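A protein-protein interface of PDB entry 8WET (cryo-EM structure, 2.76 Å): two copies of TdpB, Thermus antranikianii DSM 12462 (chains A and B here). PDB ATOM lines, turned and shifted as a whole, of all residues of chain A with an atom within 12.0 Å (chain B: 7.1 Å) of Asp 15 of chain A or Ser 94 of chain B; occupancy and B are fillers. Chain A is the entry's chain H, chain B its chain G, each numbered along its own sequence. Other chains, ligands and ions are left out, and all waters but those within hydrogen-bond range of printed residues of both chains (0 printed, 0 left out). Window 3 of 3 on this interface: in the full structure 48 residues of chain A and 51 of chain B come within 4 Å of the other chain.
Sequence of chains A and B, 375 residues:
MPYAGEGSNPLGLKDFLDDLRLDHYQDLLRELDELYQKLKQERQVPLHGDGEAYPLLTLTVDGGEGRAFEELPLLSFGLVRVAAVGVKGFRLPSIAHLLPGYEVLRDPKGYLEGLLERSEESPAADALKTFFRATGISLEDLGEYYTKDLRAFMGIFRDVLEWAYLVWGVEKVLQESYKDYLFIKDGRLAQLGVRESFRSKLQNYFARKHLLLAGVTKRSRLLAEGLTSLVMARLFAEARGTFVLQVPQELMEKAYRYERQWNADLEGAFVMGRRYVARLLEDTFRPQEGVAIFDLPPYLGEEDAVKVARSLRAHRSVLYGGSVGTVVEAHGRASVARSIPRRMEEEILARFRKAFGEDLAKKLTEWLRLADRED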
ATOM      1  N   ASP A  15      12.593  -8.909   2.806  1.00  0.00           N
ATOM      2  CA  ASP A  15      11.800  -9.613   3.806  1.00  0.00           C
ATOM      3  C   ASP A  15      10.691  -8.717   4.349  1.00  0.00           C
ATOM      4  O   ASP A  15       9.606  -8.630   3.774  1.00  0.00           O
ATOM      5  CB  ASP A  15      12.691 -10.097   4.953  1.00  0.00           C
ATOM      6  CG  ASP A  15      13.826 -10.983   4.477  1.00  0.00           C
ATOM      7  OD1 ASP A  15      13.816 -11.378   3.293  1.00  0.00           O
ATOM      8  OD2 ASP A  15      14.728 -11.282   5.287  1.00  0.00           O
ATOM      9  N   PHE A  16      10.980  -8.053   5.465  1.00  0.00           N
ATOM     10  CA  PHE A  16      10.045  -7.132   6.098  1.00  0.00           C
ATOM     11  C   PHE A  16      10.073  -5.774   5.407  1.00  0.00           C
ATOM     12  O   PHE A  16      10.545  -5.666   4.270  1.00  0.00           O
ATOM     13  CB  PHE A  16      10.350  -6.999   7.591  1.00  0.00           C
ATOM     14  CG  PHE A  16       9.882  -8.171   8.405  1.00  0.00           C
ATOM     15  CD1 PHE A  16       8.916  -9.031   7.907  1.00  0.00           C
ATOM     16  CD2 PHE A  16      10.408  -8.417   9.663  1.00  0.00           C
ATOM     17  CE1 PHE A  16       8.479 -10.113   8.649  1.00  0.00           C
ATOM     18  CE2 PHE A  16       9.975  -9.499  10.410  1.00  0.00           C
ATOM     19  CZ  PHE A  16       9.010 -10.348   9.902  1.00  0.00           C
ATOM     20  N   LEU A  17       9.536  -4.751   6.081  1.00  0.00           N
ATOM     21  CA  LEU A  17       9.375  -3.412   5.519  1.00  0.00           C
ATOM     22  C   LEU A  17      10.579  -2.976   4.687  1.00  0.00           C
ATOM     23  O   LEU A  17      10.461  -2.741   3.478  1.00  0.00           O
ATOM     24  CB  LEU A  17       9.125  -2.428   6.668  1.00  0.00           C
ATOM     25  CG  LEU A  17       8.720  -0.977   6.412  1.00  0.00           C
ATOM     26  CD1 LEU A  17       7.926  -0.484   7.600  1.00  0.00           C
ATOM     27  CD2 LEU A  17       9.932  -0.084   6.192  1.00  0.00           C
ATOM     28  N   ASP A  18      11.744  -2.877   5.324  1.00  0.00           N
ATOM     29  CA  ASP A  18      13.022  -2.673   4.642  1.00  0.00           C
ATOM     30  C   ASP A  18      12.993  -1.441   3.734  1.00  0.00           C
ATOM     31  O   ASP A  18      13.166  -1.527   2.516  1.00  0.00           O
ATOM     32  CB  ASP A  18      13.410  -3.928   3.852  1.00  0.00           C
ATOM     33  CG  ASP A  18      14.868  -3.926   3.429  1.00  0.00           C
ATOM     34  OD1 ASP A  18      15.596  -2.974   3.782  1.00  0.00           O
ATOM     35  OD2 ASP A  18      15.285  -4.880   2.740  1.00  0.00           O
ATOM     36  N   ASP A  19      12.769  -0.279   4.354  1.00  0.00           N
ATOM     37  CA  ASP A  19      12.891   1.021   3.689  1.00  0.00           C
ATOM     38  C   ASP A  19      11.966   1.106   2.468  1.00  0.00           C
ATOM     39  O   ASP A  19      12.403   1.145   1.315  1.00  0.00           O
ATOM     40  CB  ASP A  19      14.349   1.293   3.298  1.00  0.00           C
ATOM     41  CG  ASP A  19      14.684   2.771   3.286  1.00  0.00           C
ATOM     42  OD1 ASP A  19      13.804   3.580   2.930  1.00  0.00           O
ATOM     43  OD2 ASP A  19      15.832   3.123   3.633  1.00  0.00           O
ATOM     44  N   LEU A  20      10.661   1.113   2.763  1.00  0.00           N
ATOM     45  CA  LEU A  20       9.653   1.136   1.704  1.00  0.00           C
ATOM     46  C   LEU A  20       9.838   2.319   0.758  1.00  0.00           C
ATOM     47  O   LEU A  20       9.483   2.222  -0.422  1.00  0.00           O
ATOM     48  CB  LEU A  20       8.245   1.162   2.305  1.00  0.00           C
ATOM     49  CG  LEU A  20       7.723   2.443   2.968  1.00  0.00           C
ATOM     50  CD1 LEU A  20       6.215   2.363   3.145  1.00  0.00           C
ATOM     51  CD2 LEU A  20       8.395   2.711   4.307  1.00  0.00           C
ATOM     52  N   ARG A  21      10.353   3.444   1.264  1.00  0.00           N
ATOM     53  CA  ARG A  21      10.739   4.605   0.463  1.00  0.00           C
ATOM     54  C   ARG A  21       9.537   5.350  -0.110  1.00  0.00           C
ATOM     55  O   ARG A  21       8.542   4.737  -0.511  1.00  0.00           O
ATOM     56  CB  ARG A  21      11.692   4.198  -0.667  1.00  0.00           C
ATOM     57  CG  ARG A  21      13.131   3.996  -0.223  1.00  0.00           C
ATOM     58  CD  ARG A  21      14.066   3.865  -1.413  1.00  0.00           C
ATOM     59  NE  ARG A  21      13.940   2.571  -2.073  1.00  0.00           N
ATOM     60  CZ  ARG A  21      14.625   2.209  -3.149  1.00  0.00           C
ATOM     61  NH1 ARG A  21      15.500   3.023  -3.717  1.00  0.00           N
ATOM     62  NH2 ARG A  21      14.428   1.000  -3.666  1.00  0.00           N
ATOM     63  N   ARG B  81       6.258 -11.318  -3.284  1.00  0.00           N
ATOM     64  CA  ARG B  81       7.199 -11.929  -2.347  1.00  0.00           C
ATOM     65  C   ARG B  81       7.484 -13.343  -2.851  1.00  0.00           C
ATOM     66  O   ARG B  81       6.654 -14.238  -2.678  1.00  0.00           O
ATOM     67  CB  ARG B  81       6.634 -11.939  -0.936  1.00  0.00           C
ATOM     68  CG  ARG B  81       7.559 -12.541   0.107  1.00  0.00           C
ATOM     69  CD  ARG B  81       6.886 -12.588   1.468  1.00  0.00           C
ATOM     70  NE  ARG B  81       7.688 -13.305   2.453  1.00  0.00           N
ATOM     71  CZ  ARG B  81       8.559 -12.730   3.271  1.00  0.00           C
ATOM     72  NH1 ARG B  81       8.768 -11.424   3.251  1.00  0.00           N
ATOM     73  NH2 ARG B  81       9.237 -13.484   4.130  1.00  0.00           N
ATOM     74  N   VAL B  82       8.651 -13.529  -3.460  1.00  0.00           N
ATOM     75  CA  VAL B  82       9.042 -14.799  -4.062  1.00  0.00           C
ATOM     76  C   VAL B  82      10.154 -15.415  -3.222  1.00  0.00           C
ATOM     77  O   VAL B  82      11.105 -14.725  -2.832  1.00  0.00           O
ATOM     78  CB  VAL B  82       9.467 -14.617  -5.530  1.00  0.00           C
ATOM     79  CG1 VAL B  82      10.603 -13.614  -5.651  1.00  0.00           C
ATOM     80  CG2 VAL B  82       9.860 -15.952  -6.143  1.00  0.00           C
ATOM     81  N   ALA B  83      10.020 -16.705  -2.924  1.00  0.00           N
ATOM     82  CA  ALA B  83      10.970 -17.412  -2.076  1.00  0.00           C
ATOM     83  C   ALA B  83      11.169 -18.818  -2.634  1.00  0.00           C
ATOM     84  O   ALA B  83      10.669 -19.161  -3.710  1.00  0.00           O
ATOM     85  CB  ALA B  83      10.485 -17.434  -0.621  1.00  0.00           C
ATOM     86  N   ALA B  84      11.915 -19.635  -1.893  1.00  0.00           N
ATOM     87  CA  ALA B  84      12.164 -21.018  -2.270  1.00  0.00           C
ATOM     88  C   ALA B  84      12.523 -21.801  -1.016  1.00  0.00           C
ATOM     89  O   ALA B  84      12.885 -21.224   0.014  1.00  0.00           O
ATOM     90  CB  ALA B  84      13.279 -21.128  -3.316  1.00  0.00           C
ATOM     91  N   ARG B  91      17.030 -23.655   2.023  1.00  0.00           N
ATOM     92  CA  ARG B  91      16.305 -22.595   1.339  1.00  0.00           C
ATOM     93  C   ARG B  91      17.198 -21.377   1.118  1.00  0.00           C
ATOM     94  O   ARG B  91      18.096 -21.078   1.911  1.00  0.00           O
ATOM     95  CB  ARG B  91      15.053 -22.204   2.132  1.00  0.00           C
ATOM     96  CG  ARG B  91      15.259 -21.139   3.200  1.00  0.00           C
ATOM     97  CD  ARG B  91      15.997 -21.684   4.411  1.00  0.00           C
ATOM     98  NE  ARG B  91      16.135 -20.679   5.457  1.00  0.00           N
ATOM     99  CZ  ARG B  91      17.082 -19.751   5.484  1.00  0.00           C
ATOM    100  NH1 ARG B  91      17.996 -19.669   4.532  1.00  0.00           N
ATOM    101  NH2 ARG B  91      17.110 -18.882   6.490  1.00  0.00           N
ATOM    102  N   LEU B  92      16.953 -20.688   0.011  1.00  0.00           N
ATOM    103  CA  LEU B  92      17.652 -19.469  -0.357  1.00  0.00           C
ATOM    104  C   LEU B  92      16.942 -18.254   0.224  1.00  0.00           C
ATOM    105  O   LEU B  92      15.759 -18.322   0.570  1.00  0.00           O
ATOM    106  CB  LEU B  92      17.739 -19.358  -1.878  1.00  0.00           C
ATOM    107  CG  LEU B  92      18.383 -20.546  -2.596  1.00  0.00           C
ATOM    108  CD1 LEU B  92      18.590 -20.239  -4.073  1.00  0.00           C
ATOM    109  CD2 LEU B  92      19.700 -20.931  -1.935  1.00  0.00           C
ATOM    110  N   PRO B  93      17.644 -17.127   0.366  1.00  0.00           N
ATOM    111  CA  PRO B  93      16.991 -15.919   0.889  1.00  0.00           C
ATOM    112  C   PRO B  93      15.823 -15.488   0.012  1.00  0.00           C
ATOM    113  O   PRO B  93      15.880 -15.564  -1.217  1.00  0.00           O
ATOM    114  CB  PRO B  93      18.114 -14.876   0.882  1.00  0.00           C
ATOM    115  CG  PRO B  93      19.369 -15.668   0.933  1.00  0.00           C
ATOM    116  CD  PRO B  93      19.094 -16.939   0.188  1.00  0.00           C
ATOM    117  N   SER B  94      14.759 -15.027   0.664  1.00  0.00           N
ATOM    118  CA  SER B  94      13.544 -14.637  -0.035  1.00  0.00           C
ATOM    119  C   SER B  94      13.652 -13.215  -0.567  1.00  0.00           C
ATOM    120  O   SER B  94      14.383 -12.378  -0.030  1.00  0.00           O
ATOM    121  CB  SER B  94      12.335 -14.751   0.893  1.00  0.00           C
ATOM    122  OG  SER B  94      12.221 -13.608   1.723  1.00  0.00           O
ATOM    123  N   ILE B  95      12.909 -12.947  -1.638  1.00  0.00           N
ATOM    124  CA  ILE B  95      12.823 -11.622  -2.241  1.00  0.00           C
ATOM    125  C   ILE B  95      11.438 -11.062  -1.955  1.00  0.00           C
ATOM    126  O   ILE B  95      10.426 -11.697  -2.274  1.00  0.00           O
ATOM    127  CB  ILE B  95      13.104 -11.665  -3.753  1.00  0.00           C
ATOM    128  CG1 ILE B  95      14.564 -12.038  -4.016  1.00  0.00           C
ATOM    129  CG2 ILE B  95      12.769 -10.330  -4.396  1.00  0.00           C
ATOM    130  CD1 ILE B  95      15.559 -11.029  -3.494  1.00  0.00           C
ATOM    131  N   ALA B  96      11.397  -9.875  -1.358  1.00  0.00           N
ATOM    132  CA  ALA B  96      10.167  -9.213  -0.931  1.00  0.00           C
ATOM    133  C   ALA B  96      10.102  -7.809  -1.514  1.00  0.00           C
ATOM    134  O   ALA B  96       9.921  -6.820  -0.799  1.00  0.00           O
ATOM    135  CB  ALA B  96      10.063  -9.179   0.590  1.00  0.00           C
ATOM    136  N   HIS B  97      10.288  -7.723  -2.831  1.00  0.00           N
ATOM    137  CA  HIS B  97      10.401  -6.462  -3.559  1.00  0.00           C
ATOM    138  C   HIS B  97       9.394  -5.423  -3.090  1.00  0.00           C
ATOM    139  O   HIS B  97       8.192  -5.693  -3.005  1.00  0.00           O
ATOM    140  CB  HIS B  97      10.209  -6.714  -5.056  1.00  0.00           C
ATOM    141  CG  HIS B  97       9.954  -5.468  -5.846  1.00  0.00           C
ATOM    142  ND1 HIS B  97      10.967  -4.635  -6.269  1.00  0.00           N
ATOM    143  CD2 HIS B  97       8.801  -4.914  -6.291  1.00  0.00           C
ATOM    144  CE1 HIS B  97      10.451  -3.621  -6.941  1.00  0.00           C
ATOM    145  NE2 HIS B  97       9.138  -3.767  -6.968  1.00  0.00           N
ATOM    146  N   PRO B 123      18.107  -6.112  -3.629  1.00  0.00           N
ATOM    147  CA  PRO B 123      18.036  -7.576  -3.787  1.00  0.00           C
ATOM    148  C   PRO B 123      17.040  -8.011  -4.848  1.00  0.00           C
ATOM    149  O   PRO B 123      17.305  -8.963  -5.592  1.00  0.00           O
ATOM    150  CB  PRO B 123      17.623  -8.070  -2.393  1.00  0.00           C
ATOM    151  CG  PRO B 123      17.811  -6.922  -1.457  1.00  0.00           C
ATOM    152  CD  PRO B 123      18.202  -5.698  -2.218  1.00  0.00           C
ATOM    153  N   TYR B 165      14.003 -15.241 -10.003  1.00  0.00           N
ATOM    154  CA  TYR B 165      14.405 -15.923  -8.777  1.00  0.00           C
ATOM    155  C   TYR B 165      15.063 -17.264  -9.070  1.00  0.00           C
ATOM    156  O   TYR B 165      15.993 -17.668  -8.362  1.00  0.00           O
ATOM    157  CB  TYR B 165      13.191 -16.115  -7.866  1.00  0.00           C
ATOM    158  CG  TYR B 165      13.527 -16.328  -6.407  1.00  0.00           C
ATOM    159  CD1 TYR B 165      13.664 -15.253  -5.540  1.00  0.00           C
ATOM    160  CD2 TYR B 165      13.704 -17.605  -5.895  1.00  0.00           C
ATOM    161  CE1 TYR B 165      13.965 -15.447  -4.206  1.00  0.00           C
ATOM    162  CE2 TYR B 165      14.006 -17.807  -4.563  1.00  0.00           C
ATOM    163  CZ  TYR B 165      14.136 -16.725  -3.723  1.00  0.00           C
ATOM    164  OH  TYR B 165      14.438 -16.922  -2.396  1.00  0.00           O
ATOM    165  N   TRP B 168      18.535 -16.239 -10.951  1.00  0.00           N
ATOM    166  CA  TRP B 168      19.477 -15.573 -10.056  1.00  0.00           C
ATOM    167  C   TRP B 168      20.141 -16.562  -9.106  1.00  0.00           C
ATOM    168  O   TRP B 168      21.351 -16.486  -8.868  1.00  0.00           O
ATOM    169  CB  TRP B 168      18.762 -14.472  -9.272  1.00  0.00           C
ATOM    170  CG  TRP B 168      19.558 -13.915  -8.135  1.00  0.00           C
ATOM    171  CD1 TRP B 168      20.681 -13.147  -8.220  1.00  0.00           C
ATOM    172  CD2 TRP B 168      19.285 -14.076  -6.739  1.00  0.00           C
ATOM    173  NE1 TRP B 168      21.128 -12.822  -6.962  1.00  0.00           N
ATOM    174  CE2 TRP B 168      20.287 -13.380  -6.034  1.00  0.00           C
ATOM    175  CE3 TRP B 168      18.292 -14.743  -6.014  1.00  0.00           C
ATOM    176  CZ2 TRP B 168      20.325 -13.332  -4.643  1.00  0.00           C
ATOM    177  CZ3 TRP B 168      18.332 -14.694  -4.634  1.00  0.00           C
ATOM    178  CH2 TRP B 168      19.342 -13.994  -3.962  1.00  0.00           C
ATOM    179  N   ARG B 333       6.502 -20.314   3.557  1.00  0.00           N
ATOM    180  CA  ARG B 333       7.665 -19.439   3.619  1.00  0.00           C
ATOM    181  C   ARG B 333       7.566 -18.254   2.665  1.00  0.00           C
ATOM    182  O   ARG B 333       8.463 -17.406   2.661  1.00  0.00           O
ATOM    183  CB  ARG B 333       8.938 -20.240   3.320  1.00  0.00           C
ATOM    184  CG  ARG B 333      10.197 -19.705   3.989  1.00  0.00           C
ATOM    185  CD  ARG B 333      10.100 -19.760   5.507  1.00  0.00           C
ATOM    186  NE  ARG B 333       9.485 -20.994   5.979  1.00  0.00           N
ATOM    187  CZ  ARG B 333       8.993 -21.165   7.200  1.00  0.00           C
ATOM    188  NH1 ARG B 333       9.028 -20.198   8.102  1.00  0.00           N
ATOM    189  NH2 ARG B 333       8.452 -22.337   7.523  1.00  0.00           N
ATOM    190  N   ALA B 334       6.500 -18.168   1.864  1.00  0.00           N
ATOM    191  CA  ALA B 334       6.401 -17.109   0.867  1.00  0.00           C
ATOM    192  C   ALA B 334       5.006 -16.500   0.760  1.00  0.00           C
ATOM    193  O   ALA B 334       4.788 -15.653  -0.115  1.00  0.00           O
ATOM    194  CB  ALA B 334       6.835 -17.629  -0.508  1.00  0.00           C
ATOM    195  N   ARG B 343      -2.062  -3.724   8.359  1.00  0.00           N
ATOM    196  CA  ARG B 343      -0.669  -3.490   8.731  1.00  0.00           C
ATOM    197  C   ARG B 343      -0.058  -2.349   7.928  1.00  0.00           C
ATOM    198  O   ARG B 343       0.644  -1.497   8.486  1.00  0.00           O
ATOM    199  CB  ARG B 343       0.143  -4.771   8.542  1.00  0.00           C
ATOM    200  CG  ARG B 343       1.642  -4.591   8.716  1.00  0.00           C
ATOM    201  CD  ARG B 343       2.345  -5.930   8.849  1.00  0.00           C
ATOM    202  NE  ARG B 343       3.708  -5.884   8.334  1.00  0.00           N
ATOM    203  CZ  ARG B 343       4.522  -6.928   8.279  1.00  0.00           C
ATOM    204  NH1 ARG B 343       4.142  -8.124   8.701  1.00  0.00           N
ATOM    205  NH2 ARG B 343       5.749  -6.769   7.790  1.00  0.00           N
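O of Asp 15 of chain A is in hydrogen-bond range of NH1 of Arg 81 of chain B (3.0 Å).
OG of Ser 94 of chain B lies within hydrogen-bond range of OD1 of Asp 15 of chain A, at 3.2 Å.
O of Asp 15 of chain A touches CB of Ala 96 of chain B, 3.3 Å away.
Phe 16 of chain A touches Arg 343 of chain B (CD1 to NH2, 3.9 Å).
Hydrophobic or aromatic side chains of chain A within 4 Å of the printed part of chain B: Phe 16.
Of the 17 printed residues of chain B, 4 touch a printed residue of chain A.
Hydrophobic or aromatic side chains of chain B that line the printed part of chain A: Ala 96.
Along chain B the printed residues that touch a printed residue of chain A span positions 81 to 343.
Among the printed residues, 4 pairs touch across the chains.
Among the printed residues, no Asp or Glu carboxylate lies within 4 Å of a Lys or Arg side-chain nitrogen of the other chain.
Asp 15 of chain A touches just these residues of chain B: Arg 81, Ser 94 and Ala 96.
Ser 94 of chain B touches just one residue of chain A: Asp 15 (3.2 Å).
No residue of chain A comes within 4 Å of Val 82 of chain B.
Ala 83 of chain B touches none of the printed residues of chain A.
Of the printed residues of chain A, Ala 96 of chain B touches Asp 15.
Of the printed residues of chain B, Phe 16 of chain A touches Arg 343 (3.9 Å).
Printed residues of chain A within 4 Å of Arg 343 of chain B: Phe 16.
Trp 168 of chain B touches none of the printed residues of chain A.
The nearest residue of chain A that does not touch Ser 94 of chain B is Phe 16 of chain A (6.8 Å).
The nearest printed residue of chain A that does not touch Arg 81 of chain B is Phe 16 of chain A (4.6 Å).
No position is printed for both chains.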
